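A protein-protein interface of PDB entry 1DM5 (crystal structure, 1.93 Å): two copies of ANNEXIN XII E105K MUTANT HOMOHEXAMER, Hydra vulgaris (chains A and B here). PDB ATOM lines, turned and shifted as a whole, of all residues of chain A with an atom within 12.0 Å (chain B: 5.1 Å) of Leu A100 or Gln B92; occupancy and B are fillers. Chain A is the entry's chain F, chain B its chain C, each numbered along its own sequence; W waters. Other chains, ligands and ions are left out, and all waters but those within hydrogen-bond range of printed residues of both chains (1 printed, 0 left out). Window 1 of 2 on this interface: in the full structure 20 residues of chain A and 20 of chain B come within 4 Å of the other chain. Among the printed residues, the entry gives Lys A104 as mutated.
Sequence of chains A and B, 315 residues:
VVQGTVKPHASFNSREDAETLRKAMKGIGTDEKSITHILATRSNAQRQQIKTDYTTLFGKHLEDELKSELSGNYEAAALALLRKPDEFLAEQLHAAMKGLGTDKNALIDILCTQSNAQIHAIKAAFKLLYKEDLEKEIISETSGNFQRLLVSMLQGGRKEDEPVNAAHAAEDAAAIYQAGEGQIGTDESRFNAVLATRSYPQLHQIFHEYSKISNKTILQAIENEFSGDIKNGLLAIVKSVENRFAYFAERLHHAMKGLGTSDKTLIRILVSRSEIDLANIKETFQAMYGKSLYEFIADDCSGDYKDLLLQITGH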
ATOM      1  N   GLU A  91      32.351  -3.539 -15.877  1.00  0.00           N
ATOM      2  CA  GLU A  91      31.241  -4.305 -15.299  1.00  0.00           C
ATOM      3  C   GLU A  91      29.930  -3.942 -15.975  1.00  0.00           C
ATOM      4  O   GLU A  91      29.045  -4.759 -16.220  1.00  0.00           O
ATOM      5  CB  GLU A  91      31.149  -4.097 -13.780  1.00  0.00           C
ATOM      6  CG  GLU A  91      29.755  -4.322 -13.215  1.00  0.00           C
ATOM      7  CD  GLU A  91      29.526  -3.521 -11.938  1.00  0.00           C
ATOM      8  OE1 GLU A  91      29.630  -4.126 -10.851  1.00  0.00           O
ATOM      9  OE2 GLU A  91      29.247  -2.302 -12.052  1.00  0.00           O
ATOM     10  N   GLN A  92      29.772  -2.660 -16.300  1.00  0.00           N
ATOM     11  CA  GLN A  92      28.582  -2.253 -17.045  1.00  0.00           C
ATOM     12  C   GLN A  92      28.521  -2.966 -18.390  1.00  0.00           C
ATOM     13  O   GLN A  92      27.451  -3.265 -18.909  1.00  0.00           O
ATOM     14  CB  GLN A  92      28.556  -0.730 -17.213  1.00  0.00           C
ATOM     15  CG  GLN A  92      28.214  -0.024 -15.901  1.00  0.00           C
ATOM     16  CD  GLN A  92      26.750  -0.151 -15.549  1.00  0.00           C
ATOM     17  OE1 GLN A  92      25.896   0.276 -16.322  1.00  0.00           O
ATOM     18  NE2 GLN A  92      26.458  -0.761 -14.408  1.00  0.00           N
ATOM     19  N   LEU A  93      29.686  -3.307 -18.948  1.00  0.00           N
ATOM     20  CA  LEU A  93      29.647  -3.972 -20.251  1.00  0.00           C
ATOM     21  C   LEU A  93      29.122  -5.392 -20.063  1.00  0.00           C
ATOM     22  O   LEU A  93      28.193  -5.822 -20.736  1.00  0.00           O
ATOM     23  CB  LEU A  93      31.033  -4.001 -20.885  1.00  0.00           C
ATOM     24  CG  LEU A  93      31.473  -2.744 -21.628  1.00  0.00           C
ATOM     25  CD1 LEU A  93      32.894  -2.916 -22.142  1.00  0.00           C
ATOM     26  CD2 LEU A  93      30.517  -2.417 -22.763  1.00  0.00           C
ATOM     27  N   HIS A  94      29.755  -6.056 -19.104  1.00  0.00           N
ATOM     28  CA  HIS A  94      29.416  -7.434 -18.768  1.00  0.00           C
ATOM     29  C   HIS A  94      27.915  -7.581 -18.577  1.00  0.00           C
ATOM     30  O   HIS A  94      27.261  -8.396 -19.231  1.00  0.00           O
ATOM     31  CB  HIS A  94      30.164  -7.811 -17.490  1.00  0.00           C
ATOM     32  CG  HIS A  94      30.212  -9.282 -17.240  1.00  0.00           C
ATOM     33  ND1 HIS A  94      31.106 -10.111 -17.875  1.00  0.00           N
ATOM     34  CD2 HIS A  94      29.492 -10.073 -16.415  1.00  0.00           C
ATOM     35  CE1 HIS A  94      30.936 -11.352 -17.463  1.00  0.00           C
ATOM     36  NE2 HIS A  94      29.955 -11.359 -16.576  1.00  0.00           N
ATOM     37  N   ALA A  95      27.360  -6.746 -17.707  1.00  0.00           N
ATOM     38  CA  ALA A  95      25.934  -6.787 -17.409  1.00  0.00           C
ATOM     39  C   ALA A  95      25.095  -6.471 -18.636  1.00  0.00           C
ATOM     40  O   ALA A  95      23.943  -6.906 -18.741  1.00  0.00           O
ATOM     41  CB  ALA A  95      25.586  -5.828 -16.285  1.00  0.00           C
ATOM     42  N   ALA A  96      25.648  -5.716 -19.589  1.00  0.00           N
ATOM     43  CA  ALA A  96      24.862  -5.487 -20.803  1.00  0.00           C
ATOM     44  C   ALA A  96      24.816  -6.743 -21.683  1.00  0.00           C
ATOM     45  O   ALA A  96      23.971  -6.840 -22.575  1.00  0.00           O
ATOM     46  CB  ALA A  96      25.419  -4.328 -21.615  1.00  0.00           C
ATOM     47  N   MET A  97      25.728  -7.676 -21.448  1.00  0.00           N
ATOM     48  CA  MET A  97      25.907  -8.827 -22.321  1.00  0.00           C
ATOM     49  C   MET A  97      25.432 -10.138 -21.699  1.00  0.00           C
ATOM     50  O   MET A  97      24.817 -10.970 -22.361  1.00  0.00           O
ATOM     51  CB  MET A  97      27.393  -9.027 -22.668  1.00  0.00           C
ATOM     52  CG  MET A  97      27.988  -8.015 -23.620  1.00  0.00           C
ATOM     53  SD  MET A  97      29.693  -8.355 -24.064  1.00  0.00           S
ATOM     54  CE  MET A  97      30.550  -8.421 -22.509  1.00  0.00           C
ATOM     55  N   LYS A  98      25.830 -10.346 -20.456  1.00  0.00           N
ATOM     56  CA  LYS A  98      25.731 -11.620 -19.772  1.00  0.00           C
ATOM     57  C   LYS A  98      24.417 -11.810 -19.031  1.00  0.00           C
ATOM     58  O   LYS A  98      24.156 -12.906 -18.524  1.00  0.00           O
ATOM     59  CB  LYS A  98      26.937 -11.704 -18.838  1.00  0.00           C
ATOM     60  CG  LYS A  98      28.255 -11.971 -19.553  1.00  0.00           C
ATOM     61  CD  LYS A  98      27.928 -12.236 -21.027  1.00  0.00           C
ATOM     62  CE  LYS A  98      29.171 -12.342 -21.880  1.00  0.00           C
ATOM     63  NZ  LYS A  98      29.045 -13.330 -22.988  1.00  0.00           N
ATOM     64  N   GLY A  99      23.570 -10.783 -18.988  1.00  0.00           N
ATOM     65  CA  GLY A  99      22.245 -10.947 -18.405  1.00  0.00           C
ATOM     66  C   GLY A  99      21.322 -11.677 -19.367  1.00  0.00           C
ATOM     67  O   GLY A  99      21.798 -12.246 -20.354  1.00  0.00           O
ATOM     68  N   LEU A 100      20.019 -11.651 -19.127  1.00  0.00           N
ATOM     69  CA  LEU A 100      19.052 -12.320 -20.004  1.00  0.00           C
ATOM     70  C   LEU A 100      19.169 -11.818 -21.438  1.00  0.00           C
ATOM     71  O   LEU A 100      19.750 -12.538 -22.247  1.00  0.00           O
ATOM     72  CB  LEU A 100      17.648 -12.149 -19.457  1.00  0.00           C
ATOM     73  CG  LEU A 100      16.597 -13.227 -19.645  1.00  0.00           C
ATOM     74  CD1 LEU A 100      15.207 -12.609 -19.709  1.00  0.00           C
ATOM     75  CD2 LEU A 100      16.852 -14.091 -20.871  1.00  0.00           C
ATOM     76  N   GLY A 101      18.653 -10.651 -21.808  1.00  0.00           N
ATOM     77  CA  GLY A 101      18.809 -10.211 -23.192  1.00  0.00           C
ATOM     78  C   GLY A 101      20.102  -9.449 -23.401  1.00  0.00           C
ATOM     79  O   GLY A 101      21.094  -9.662 -22.698  1.00  0.00           O
ATOM     80  N   THR A 102      20.117  -8.539 -24.373  1.00  0.00           N
ATOM     81  CA  THR A 102      21.310  -7.729 -24.615  1.00  0.00           C
ATOM     82  C   THR A 102      20.960  -6.250 -24.540  1.00  0.00           C
ATOM     83  O   THR A 102      20.104  -5.785 -25.292  1.00  0.00           O
ATOM     84  CB  THR A 102      21.964  -8.076 -25.962  1.00  0.00           C
ATOM     85  OG1 THR A 102      22.359  -9.460 -25.949  1.00  0.00           O
ATOM     86  CG2 THR A 102      23.250  -7.291 -26.193  1.00  0.00           C
ATOM     87  N   ASP A 103      21.595  -5.517 -23.624  1.00  0.00           N
ATOM     88  CA  ASP A 103      21.413  -4.073 -23.549  1.00  0.00           C
ATOM     89  C   ASP A 103      22.314  -3.395 -24.585  1.00  0.00           C
ATOM     90  O   ASP A 103      23.416  -2.937 -24.284  1.00  0.00           O
ATOM     91  CB  ASP A 103      21.764  -3.511 -22.174  1.00  0.00           C
ATOM     92  CG  ASP A 103      21.231  -2.111 -21.957  1.00  0.00           C
ATOM     93  OD1 ASP A 103      21.065  -1.715 -20.778  1.00  0.00           O
ATOM     94  OD2 ASP A 103      20.946  -1.400 -22.945  1.00  0.00           O
ATOM     95  N   LYS A 104      21.834  -3.347 -25.818  1.00  0.00           N
ATOM     96  CA  LYS A 104      22.611  -2.787 -26.918  1.00  0.00           C
ATOM     97  C   LYS A 104      22.872  -1.306 -26.778  1.00  0.00           C
ATOM     98  O   LYS A 104      24.003  -0.860 -26.974  1.00  0.00           O
ATOM     99  CB  LYS A 104      21.908  -3.161 -28.236  1.00  0.00           C
ATOM    100  CG  LYS A 104      21.755  -4.683 -28.271  1.00  0.00           C
ATOM    101  CD  LYS A 104      21.060  -5.160 -29.524  1.00  0.00           C
ATOM    102  CE  LYS A 104      19.558  -5.290 -29.307  1.00  0.00           C
ATOM    103  NZ  LYS A 104      18.995  -6.247 -30.295  1.00  0.00           N
ATOM    104  N   LEU A 107      25.818  -0.821 -24.679  1.00  0.00           N
ATOM    105  CA  LEU A 107      27.031  -1.110 -25.437  1.00  0.00           C
ATOM    106  C   LEU A 107      27.421   0.079 -26.310  1.00  0.00           C
ATOM    107  O   LEU A 107      28.609   0.342 -26.514  1.00  0.00           O
ATOM    108  CB  LEU A 107      26.838  -2.375 -26.280  1.00  0.00           C
ATOM    109  CG  LEU A 107      26.548  -3.678 -25.531  1.00  0.00           C
ATOM    110  CD1 LEU A 107      26.522  -4.876 -26.473  1.00  0.00           C
ATOM    111  CD2 LEU A 107      27.538  -3.930 -24.401  1.00  0.00           C
ATOM    112  N   GLU A 137      33.751 -11.687 -25.926  1.00  0.00           N
ATOM    113  CA  GLU A 137      32.393 -11.740 -25.385  1.00  0.00           C
ATOM    114  C   GLU A 137      31.440 -10.945 -26.253  1.00  0.00           C
ATOM    115  O   GLU A 137      30.306 -11.345 -26.476  1.00  0.00           O
ATOM    116  CB  GLU A 137      32.399 -11.236 -23.941  1.00  0.00           C
ATOM    117  CG  GLU A 137      33.071 -12.205 -22.974  1.00  0.00           C
ATOM    118  CD  GLU A 137      32.573 -13.635 -23.140  1.00  0.00           C
ATOM    119  OE1 GLU A 137      31.628 -14.034 -22.429  1.00  0.00           O
ATOM    120  OE2 GLU A 137      33.135 -14.343 -24.004  1.00  0.00           O
ATOM    121  N   SER A 140      30.202 -12.785 -29.249  1.00  0.00           N
ATOM    122  CA  SER A 140      29.250 -13.826 -28.912  1.00  0.00           C
ATOM    123  C   SER A 140      27.861 -13.307 -28.599  1.00  0.00           C
ATOM    124  O   SER A 140      26.924 -14.106 -28.461  1.00  0.00           O
ATOM    125  CB  SER A 140      29.796 -14.663 -27.747  1.00  0.00           C
ATOM    126  OG  SER A 140      29.488 -14.085 -26.486  1.00  0.00           O
ATOM    127  N   GLU A 141      27.652 -12.005 -28.433  1.00  0.00           N
ATOM    128  CA  GLU A 141      26.316 -11.541 -28.025  1.00  0.00           C
ATOM    129  C   GLU A 141      25.696 -10.581 -29.026  1.00  0.00           C
ATOM    130  O   GLU A 141      24.600 -10.032 -28.858  1.00  0.00           O
ATOM    131  CB  GLU A 141      26.418 -10.858 -26.652  1.00  0.00           C
ATOM    132  CG  GLU A 141      25.326 -11.409 -25.657  1.00  0.00           C
ATOM    133  CD  GLU A 141      25.559 -12.849 -25.196  1.00  0.00           C
ATOM    134  OE1 GLU A 141      26.596 -13.138 -24.486  1.00  0.00           O
ATOM    135  OE2 GLU A 141      24.719 -13.772 -25.519  1.00  0.00           O
ATOM    136  N   THR A 142      26.431 -10.315 -30.101  1.00  0.00           N
ATOM    137  CA  THR A 142      25.986  -9.418 -31.155  1.00  0.00           C
ATOM    138  C   THR A 142      26.361 -10.044 -32.505  1.00  0.00           C
ATOM    139  O   THR A 142      27.213 -10.929 -32.586  1.00  0.00           O
ATOM    140  CB  THR A 142      26.668  -8.032 -31.088  1.00  0.00           C
ATOM    141  OG1 THR A 142      28.082  -8.250 -31.204  1.00  0.00           O
ATOM    142  CG2 THR A 142      26.420  -7.338 -29.765  1.00  0.00           C
ATOM    143  N   LYS A 264      19.450   1.990 -14.812  1.00  0.00           N
ATOM    144  CA  LYS A 264      20.836   1.584 -15.056  1.00  0.00           C
ATOM    145  C   LYS A 264      21.550   2.589 -15.948  1.00  0.00           C
ATOM    146  O   LYS A 264      22.733   2.868 -15.764  1.00  0.00           O
ATOM    147  CB  LYS A 264      20.871   0.185 -15.659  1.00  0.00           C
ATOM    148  CG  LYS A 264      20.657  -0.920 -14.634  1.00  0.00           C
ATOM    149  CD  LYS A 264      20.373  -2.246 -15.301  1.00  0.00           C
ATOM    150  CE  LYS A 264      19.094  -2.889 -14.749  1.00  0.00           C
ATOM    151  NZ  LYS A 264      18.108  -3.174 -15.846  1.00  0.00           N
ATOM    152  N   ALA B  76      13.925  -9.724 -24.169  1.00  0.00           N
ATOM    153  CA  ALA B  76      14.155 -10.466 -22.942  1.00  0.00           C
ATOM    154  C   ALA B  76      13.148 -11.597 -22.773  1.00  0.00           C
ATOM    155  O   ALA B  76      13.553 -12.707 -22.441  1.00  0.00           O
ATOM    156  CB  ALA B  76      14.133  -9.514 -21.753  1.00  0.00           C
ATOM    157  N   ALA B  77      11.860 -11.338 -22.970  1.00  0.00           N
ATOM    158  CA  ALA B  77      10.861 -12.388 -22.730  1.00  0.00           C
ATOM    159  C   ALA B  77      10.964 -13.518 -23.739  1.00  0.00           C
ATOM    160  O   ALA B  77      10.921 -14.705 -23.402  1.00  0.00           O
ATOM    161  CB  ALA B  77       9.461 -11.772 -22.702  1.00  0.00           C
ATOM    162  N   LEU B  79      13.616 -14.517 -25.369  1.00  0.00           N
ATOM    163  CA  LEU B  79      14.833 -15.271 -25.068  1.00  0.00           C
ATOM    164  C   LEU B  79      14.589 -16.168 -23.859  1.00  0.00           C
ATOM    165  O   LEU B  79      15.064 -17.285 -23.685  1.00  0.00           O
ATOM    166  CB  LEU B  79      15.960 -14.276 -24.753  1.00  0.00           C
ATOM    167  CG  LEU B  79      17.150 -14.162 -25.700  1.00  0.00           C
ATOM    168  CD1 LEU B  79      16.878 -14.668 -27.106  1.00  0.00           C
ATOM    169  CD2 LEU B  79      17.679 -12.733 -25.747  1.00  0.00           C
ATOM    170  N   ALA B  80      13.818 -15.603 -22.937  1.00  0.00           N
ATOM    171  CA  ALA B  80      13.501 -16.358 -21.723  1.00  0.00           C
ATOM    172  C   ALA B  80      12.720 -17.596 -22.164  1.00  0.00           C
ATOM    173  O   ALA B  80      12.904 -18.702 -21.659  1.00  0.00           O
ATOM    174  CB  ALA B  80      12.656 -15.467 -20.834  1.00  0.00           C
ATOM    175  N   GLU B  87      18.054 -24.075 -17.144  1.00  0.00           N
ATOM    176  CA  GLU B  87      19.006 -23.098 -17.645  1.00  0.00           C
ATOM    177  C   GLU B  87      18.497 -21.679 -17.415  1.00  0.00           C
ATOM    178  O   GLU B  87      19.276 -20.810 -17.012  1.00  0.00           O
ATOM    179  CB  GLU B  87      19.318 -23.306 -19.131  1.00  0.00           C
ATOM    180  CG  GLU B  87      19.312 -24.744 -19.598  1.00  0.00           C
ATOM    181  CD  GLU B  87      20.629 -25.208 -20.213  1.00  0.00           C
ATOM    182  OE1 GLU B  87      21.335 -26.056 -19.595  1.00  0.00           O
ATOM    183  OE2 GLU B  87      20.943 -24.724 -21.330  1.00  0.00           O
ATOM    184  N   PHE B  88      17.221 -21.438 -17.689  1.00  0.00           N
ATOM    185  CA  PHE B  88      16.641 -20.110 -17.499  1.00  0.00           C
ATOM    186  C   PHE B  88      16.792 -19.656 -16.047  1.00  0.00           C
ATOM    187  O   PHE B  88      17.020 -18.492 -15.712  1.00  0.00           O
ATOM    188  CB  PHE B  88      15.166 -20.115 -17.910  1.00  0.00           C
ATOM    189  CG  PHE B  88      14.445 -18.795 -17.640  1.00  0.00           C
ATOM    190  CD1 PHE B  88      14.876 -17.615 -18.222  1.00  0.00           C
ATOM    191  CD2 PHE B  88      13.345 -18.736 -16.799  1.00  0.00           C
ATOM    192  CE1 PHE B  88      14.227 -16.419 -17.955  1.00  0.00           C
ATOM    193  CE2 PHE B  88      12.701 -17.542 -16.518  1.00  0.00           C
ATOM    194  CZ  PHE B  88      13.152 -16.369 -17.087  1.00  0.00           C
ATOM    195  N   LEU B  89      16.664 -20.596 -15.107  1.00  0.00           N
ATOM    196  CA  LEU B  89      16.741 -20.173 -13.705  1.00  0.00           C
ATOM    197  C   LEU B  89      18.169 -19.930 -13.256  1.00  0.00           C
ATOM    198  O   LEU B  89      18.415 -18.960 -12.525  1.00  0.00           O
ATOM    199  CB  LEU B  89      15.996 -21.171 -12.819  1.00  0.00           C
ATOM    200  CG  LEU B  89      14.480 -21.185 -13.089  1.00  0.00           C
ATOM    201  CD1 LEU B  89      13.820 -22.353 -12.373  1.00  0.00           C
ATOM    202  CD2 LEU B  89      13.863 -19.850 -12.679  1.00  0.00           C
ATOM    203  N   ALA B  90      19.080 -20.778 -13.724  1.00  0.00           N
ATOM    204  CA  ALA B  90      20.502 -20.622 -13.444  1.00  0.00           C
ATOM    205  C   ALA B  90      20.984 -19.251 -13.911  1.00  0.00           C
ATOM    206  O   ALA B  90      21.843 -18.641 -13.283  1.00  0.00           O
ATOM    207  CB  ALA B  90      21.327 -21.717 -14.096  1.00  0.00           C
ATOM    208  N   GLU B  91      20.412 -18.792 -15.020  1.00  0.00           N
ATOM    209  CA  GLU B  91      20.821 -17.512 -15.588  1.00  0.00           C
ATOM    210  C   GLU B  91      20.131 -16.369 -14.868  1.00  0.00           C
ATOM    211  O   GLU B  91      20.674 -15.285 -14.658  1.00  0.00           O
ATOM    212  CB  GLU B  91      20.558 -17.469 -17.089  1.00  0.00           C
ATOM    213  CG  GLU B  91      20.727 -16.075 -17.687  1.00  0.00           C
ATOM    214  CD  GLU B  91      20.018 -15.998 -19.030  1.00  0.00           C
ATOM    215  OE1 GLU B  91      20.723 -15.763 -20.034  1.00  0.00           O
ATOM    216  OE2 GLU B  91      18.783 -16.189 -19.057  1.00  0.00           O
ATOM    217  N   GLN B  92      18.920 -16.643 -14.375  1.00  0.00           N
ATOM    218  CA  GLN B  92      18.300 -15.603 -13.534  1.00  0.00           C
ATOM    219  C   GLN B  92      19.143 -15.383 -12.282  1.00  0.00           C
ATOM    220  O   GLN B  92      19.385 -14.255 -11.884  1.00  0.00           O
ATOM    221  CB  GLN B  92      16.854 -15.973 -13.186  1.00  0.00           C
ATOM    222  CG  GLN B  92      15.927 -15.861 -14.394  1.00  0.00           C
ATOM    223  CD  GLN B  92      15.830 -14.431 -14.886  1.00  0.00           C
ATOM    224  OE1 GLN B  92      15.186 -13.606 -14.243  1.00  0.00           O
ATOM    225  NE2 GLN B  92      16.519 -14.121 -15.980  1.00  0.00           N
ATOM    226  N   LEU B  93      19.643 -16.463 -11.692  1.00  0.00           N
ATOM    227  CA  LEU B  93      20.494 -16.374 -10.509  1.00  0.00           C
ATOM    228  C   LEU B  93      21.772 -15.611 -10.837  1.00  0.00           C
ATOM    229  O   LEU B  93      22.132 -14.686 -10.108  1.00  0.00           O
ATOM    230  CB  LEU B  93      20.840 -17.786 -10.018  1.00  0.00           C
ATOM    231  CG  LEU B  93      19.709 -18.497  -9.264  1.00  0.00           C
ATOM    232  CD1 LEU B  93      19.965 -19.992  -9.153  1.00  0.00           C
ATOM    233  CD2 LEU B  93      19.538 -17.880  -7.884  1.00  0.00           C
ATOM    234  N   HIS B  94      22.410 -16.041 -11.923  1.00  0.00           N
ATOM    235  CA  HIS B  94      23.657 -15.444 -12.379  1.00  0.00           C
ATOM    236  C   HIS B  94      23.504 -13.936 -12.514  1.00  0.00           C
ATOM    237  O   HIS B  94      24.319 -13.176 -11.996  1.00  0.00           O
ATOM    238  CB  HIS B  94      24.100 -16.032 -13.728  1.00  0.00           C
ATOM    239  CG  HIS B  94      25.510 -15.662 -14.090  1.00  0.00           C
ATOM    240  ND1 HIS B  94      26.596 -16.296 -13.524  1.00  0.00           N
ATOM    241  CD2 HIS B  94      26.029 -14.708 -14.895  1.00  0.00           C
ATOM    242  CE1 HIS B  94      27.717 -15.770 -13.989  1.00  0.00           C
ATOM    243  NE2 HIS B  94      27.400 -14.801 -14.822  1.00  0.00           N
ATOM    244  N   ALA B  95      22.444 -13.509 -13.192  1.00  0.00           N
ATOM    245  CA  ALA B  95      22.208 -12.081 -13.381  1.00  0.00           C
ATOM    246  C   ALA B  95      21.895 -11.387 -12.060  1.00  0.00           C
ATOM    247  O   ALA B  95      22.198 -10.211 -11.856  1.00  0.00           O
ATOM    248  CB  ALA B  95      21.081 -11.862 -14.381  1.00  0.00           C
ATOM    249  N   ALA B  96      21.272 -12.109 -11.135  1.00  0.00           N
ATOM    250  CA  ALA B  96      20.907 -11.510  -9.860  1.00  0.00           C
ATOM    251  C   ALA B  96      22.139 -11.166  -9.030  1.00  0.00           C
ATOM    252  O   ALA B  96      22.058 -10.282  -8.177  1.00  0.00           O
ATOM    253  CB  ALA B  96      19.979 -12.439  -9.079  1.00  0.00           C
ATOM    254  N   ILE B 110      13.841 -17.659  -6.198  1.00  0.00           N
ATOM    255  CA  ILE B 110      14.344 -18.860  -6.852  1.00  0.00           C
ATOM    256  C   ILE B 110      14.812 -19.911  -5.870  1.00  0.00           C
ATOM    257  O   ILE B 110      14.511 -21.098  -6.037  1.00  0.00           O
ATOM    258  CB  ILE B 110      15.463 -18.495  -7.842  1.00  0.00           C
ATOM    259  CG1 ILE B 110      15.040 -17.428  -8.863  1.00  0.00           C
ATOM    260  CG2 ILE B 110      16.003 -19.737  -8.539  1.00  0.00           C
ATOM    261  CD1 ILE B 110      16.164 -16.977  -9.782  1.00  0.00           C
ATOM    262  N   LYS B 264      11.738  -7.693 -14.874  1.00  0.00           N
ATOM    263  CA  LYS B 264      12.594  -8.818 -14.529  1.00  0.00           C
ATOM    264  C   LYS B 264      11.781  -9.895 -13.813  1.00  0.00           C
ATOM    265  O   LYS B 264      11.771 -11.057 -14.204  1.00  0.00           O
ATOM    266  CB  LYS B 264      13.733  -8.359 -13.617  1.00  0.00           C
ATOM    267  CG  LYS B 264      14.925  -7.751 -14.338  1.00  0.00           C
ATOM    268  CD  LYS B 264      15.911  -7.186 -13.326  1.00  0.00           C
ATOM    269  CE  LYS B 264      17.234  -6.817 -13.982  1.00  0.00           C
ATOM    270  NZ  LYS B 264      18.407  -7.564 -13.363  1.00  0.00           N
ATOM    271  N   ILE B 267       8.577 -11.259 -16.070  1.00  0.00           N
ATOM    272  CA  ILE B 267       8.979 -12.280 -17.036  1.00  0.00           C
ATOM    273  C   ILE B 267       9.394 -13.584 -16.371  1.00  0.00           C
ATOM    274  O   ILE B 267       9.055 -14.696 -16.789  1.00  0.00           O
ATOM    275  CB  ILE B 267      10.150 -11.782 -17.909  1.00  0.00           C
ATOM    276  CG1 ILE B 267       9.744 -10.790 -19.004  1.00  0.00           C
ATOM    277  CG2 ILE B 267      10.944 -12.924 -18.518  1.00  0.00           C
ATOM    278  CD1 ILE B 267      10.898  -9.886 -19.402  1.00  0.00           C
ATOM    279  N   ARG B 268      10.205 -13.472 -15.316  1.00  0.00           N
ATOM    280  CA  ARG B 268      10.702 -14.683 -14.670  1.00  0.00           C
ATOM    281  C   ARG B 268       9.564 -15.571 -14.181  1.00  0.00           C
ATOM    282  O   ARG B 268       9.597 -16.787 -14.373  1.00  0.00           O
ATOM    283  CB  ARG B 268      11.622 -14.334 -13.495  1.00  0.00           C
ATOM    284  CG  ARG B 268      12.229 -15.546 -12.824  1.00  0.00           C
ATOM    285  CD  ARG B 268      13.314 -15.124 -11.843  1.00  0.00           C
ATOM    286  NE  ARG B 268      12.764 -14.333 -10.747  1.00  0.00           N
ATOM    287  CZ  ARG B 268      13.025 -13.052 -10.513  1.00  0.00           C
ATOM    288  NH1 ARG B 268      13.842 -12.367 -11.305  1.00  0.00           N
ATOM    289  NH2 ARG B 268      12.439 -12.463  -9.476  1.00  0.00           N
HETATM  290  O   HOH W   1      20.122 -14.950 -22.525  1.00  0.00           O
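Water W1 lies within hydrogen-bond range of O of Leu A100 (2.5 Å) and OE1 of Glu B91 (2.7 Å).
The guanidinium group of Arg B268 sits close to the side-chain amide oxygen of Gln B92.
Printed residues of chain B within 4 Å of Leu A100: Ala B76, Leu B79, Ala B80, Glu B91 and Gln B92. Ala B76 touches just one residue of chain A: Leu A100 (3.2 Å). No residue of chain A comes within 4 Å of Ala B77. No residue of chain A comes within 4 Å of Leu B89. No residue of chain A comes within 4 Å of Leu B93. Ile B267 touches none of the printed residues of chain A. No residue of chain A comes within 4 Å of Arg B268. Of the printed residues of chain A, Leu B79 touches Leu A100 and Gly A101. Of the printed residues of chain B, Gly A99 touches Glu B91 (3.7 Å). Lys A98 touches none of the printed residues of chain B.
7 positions are printed for both chains.
Among the printed residues, merely in contact across the chains: Gly A99 with Glu B91 (3.7 Å), Leu A100 with Ala B76 (3.2 Å), Leu A100 with Leu B79 (3.99 Å), Leu A100 with Ala B80 (3.97 Å), Leu A100 with Glu B91 (3.4 Å), Leu A100 with Gln B92 (3.8 Å) and Gly A101 with Leu B79 (3.8 Å).
Of the 18 printed residues of chain B, 5 touch a printed residue of chain A. Printed residues of chain B that touch a printed residue of chain A: Ala B76, Leu B79, Ala B80, Glu B91 and Gln B92. Among the printed residues, 7 pairs touch across the chains. Among the printed residues, no Asp or Glu carboxylate lies within 4 Å of a Lys or Arg side-chain nitrogen of the other chain.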
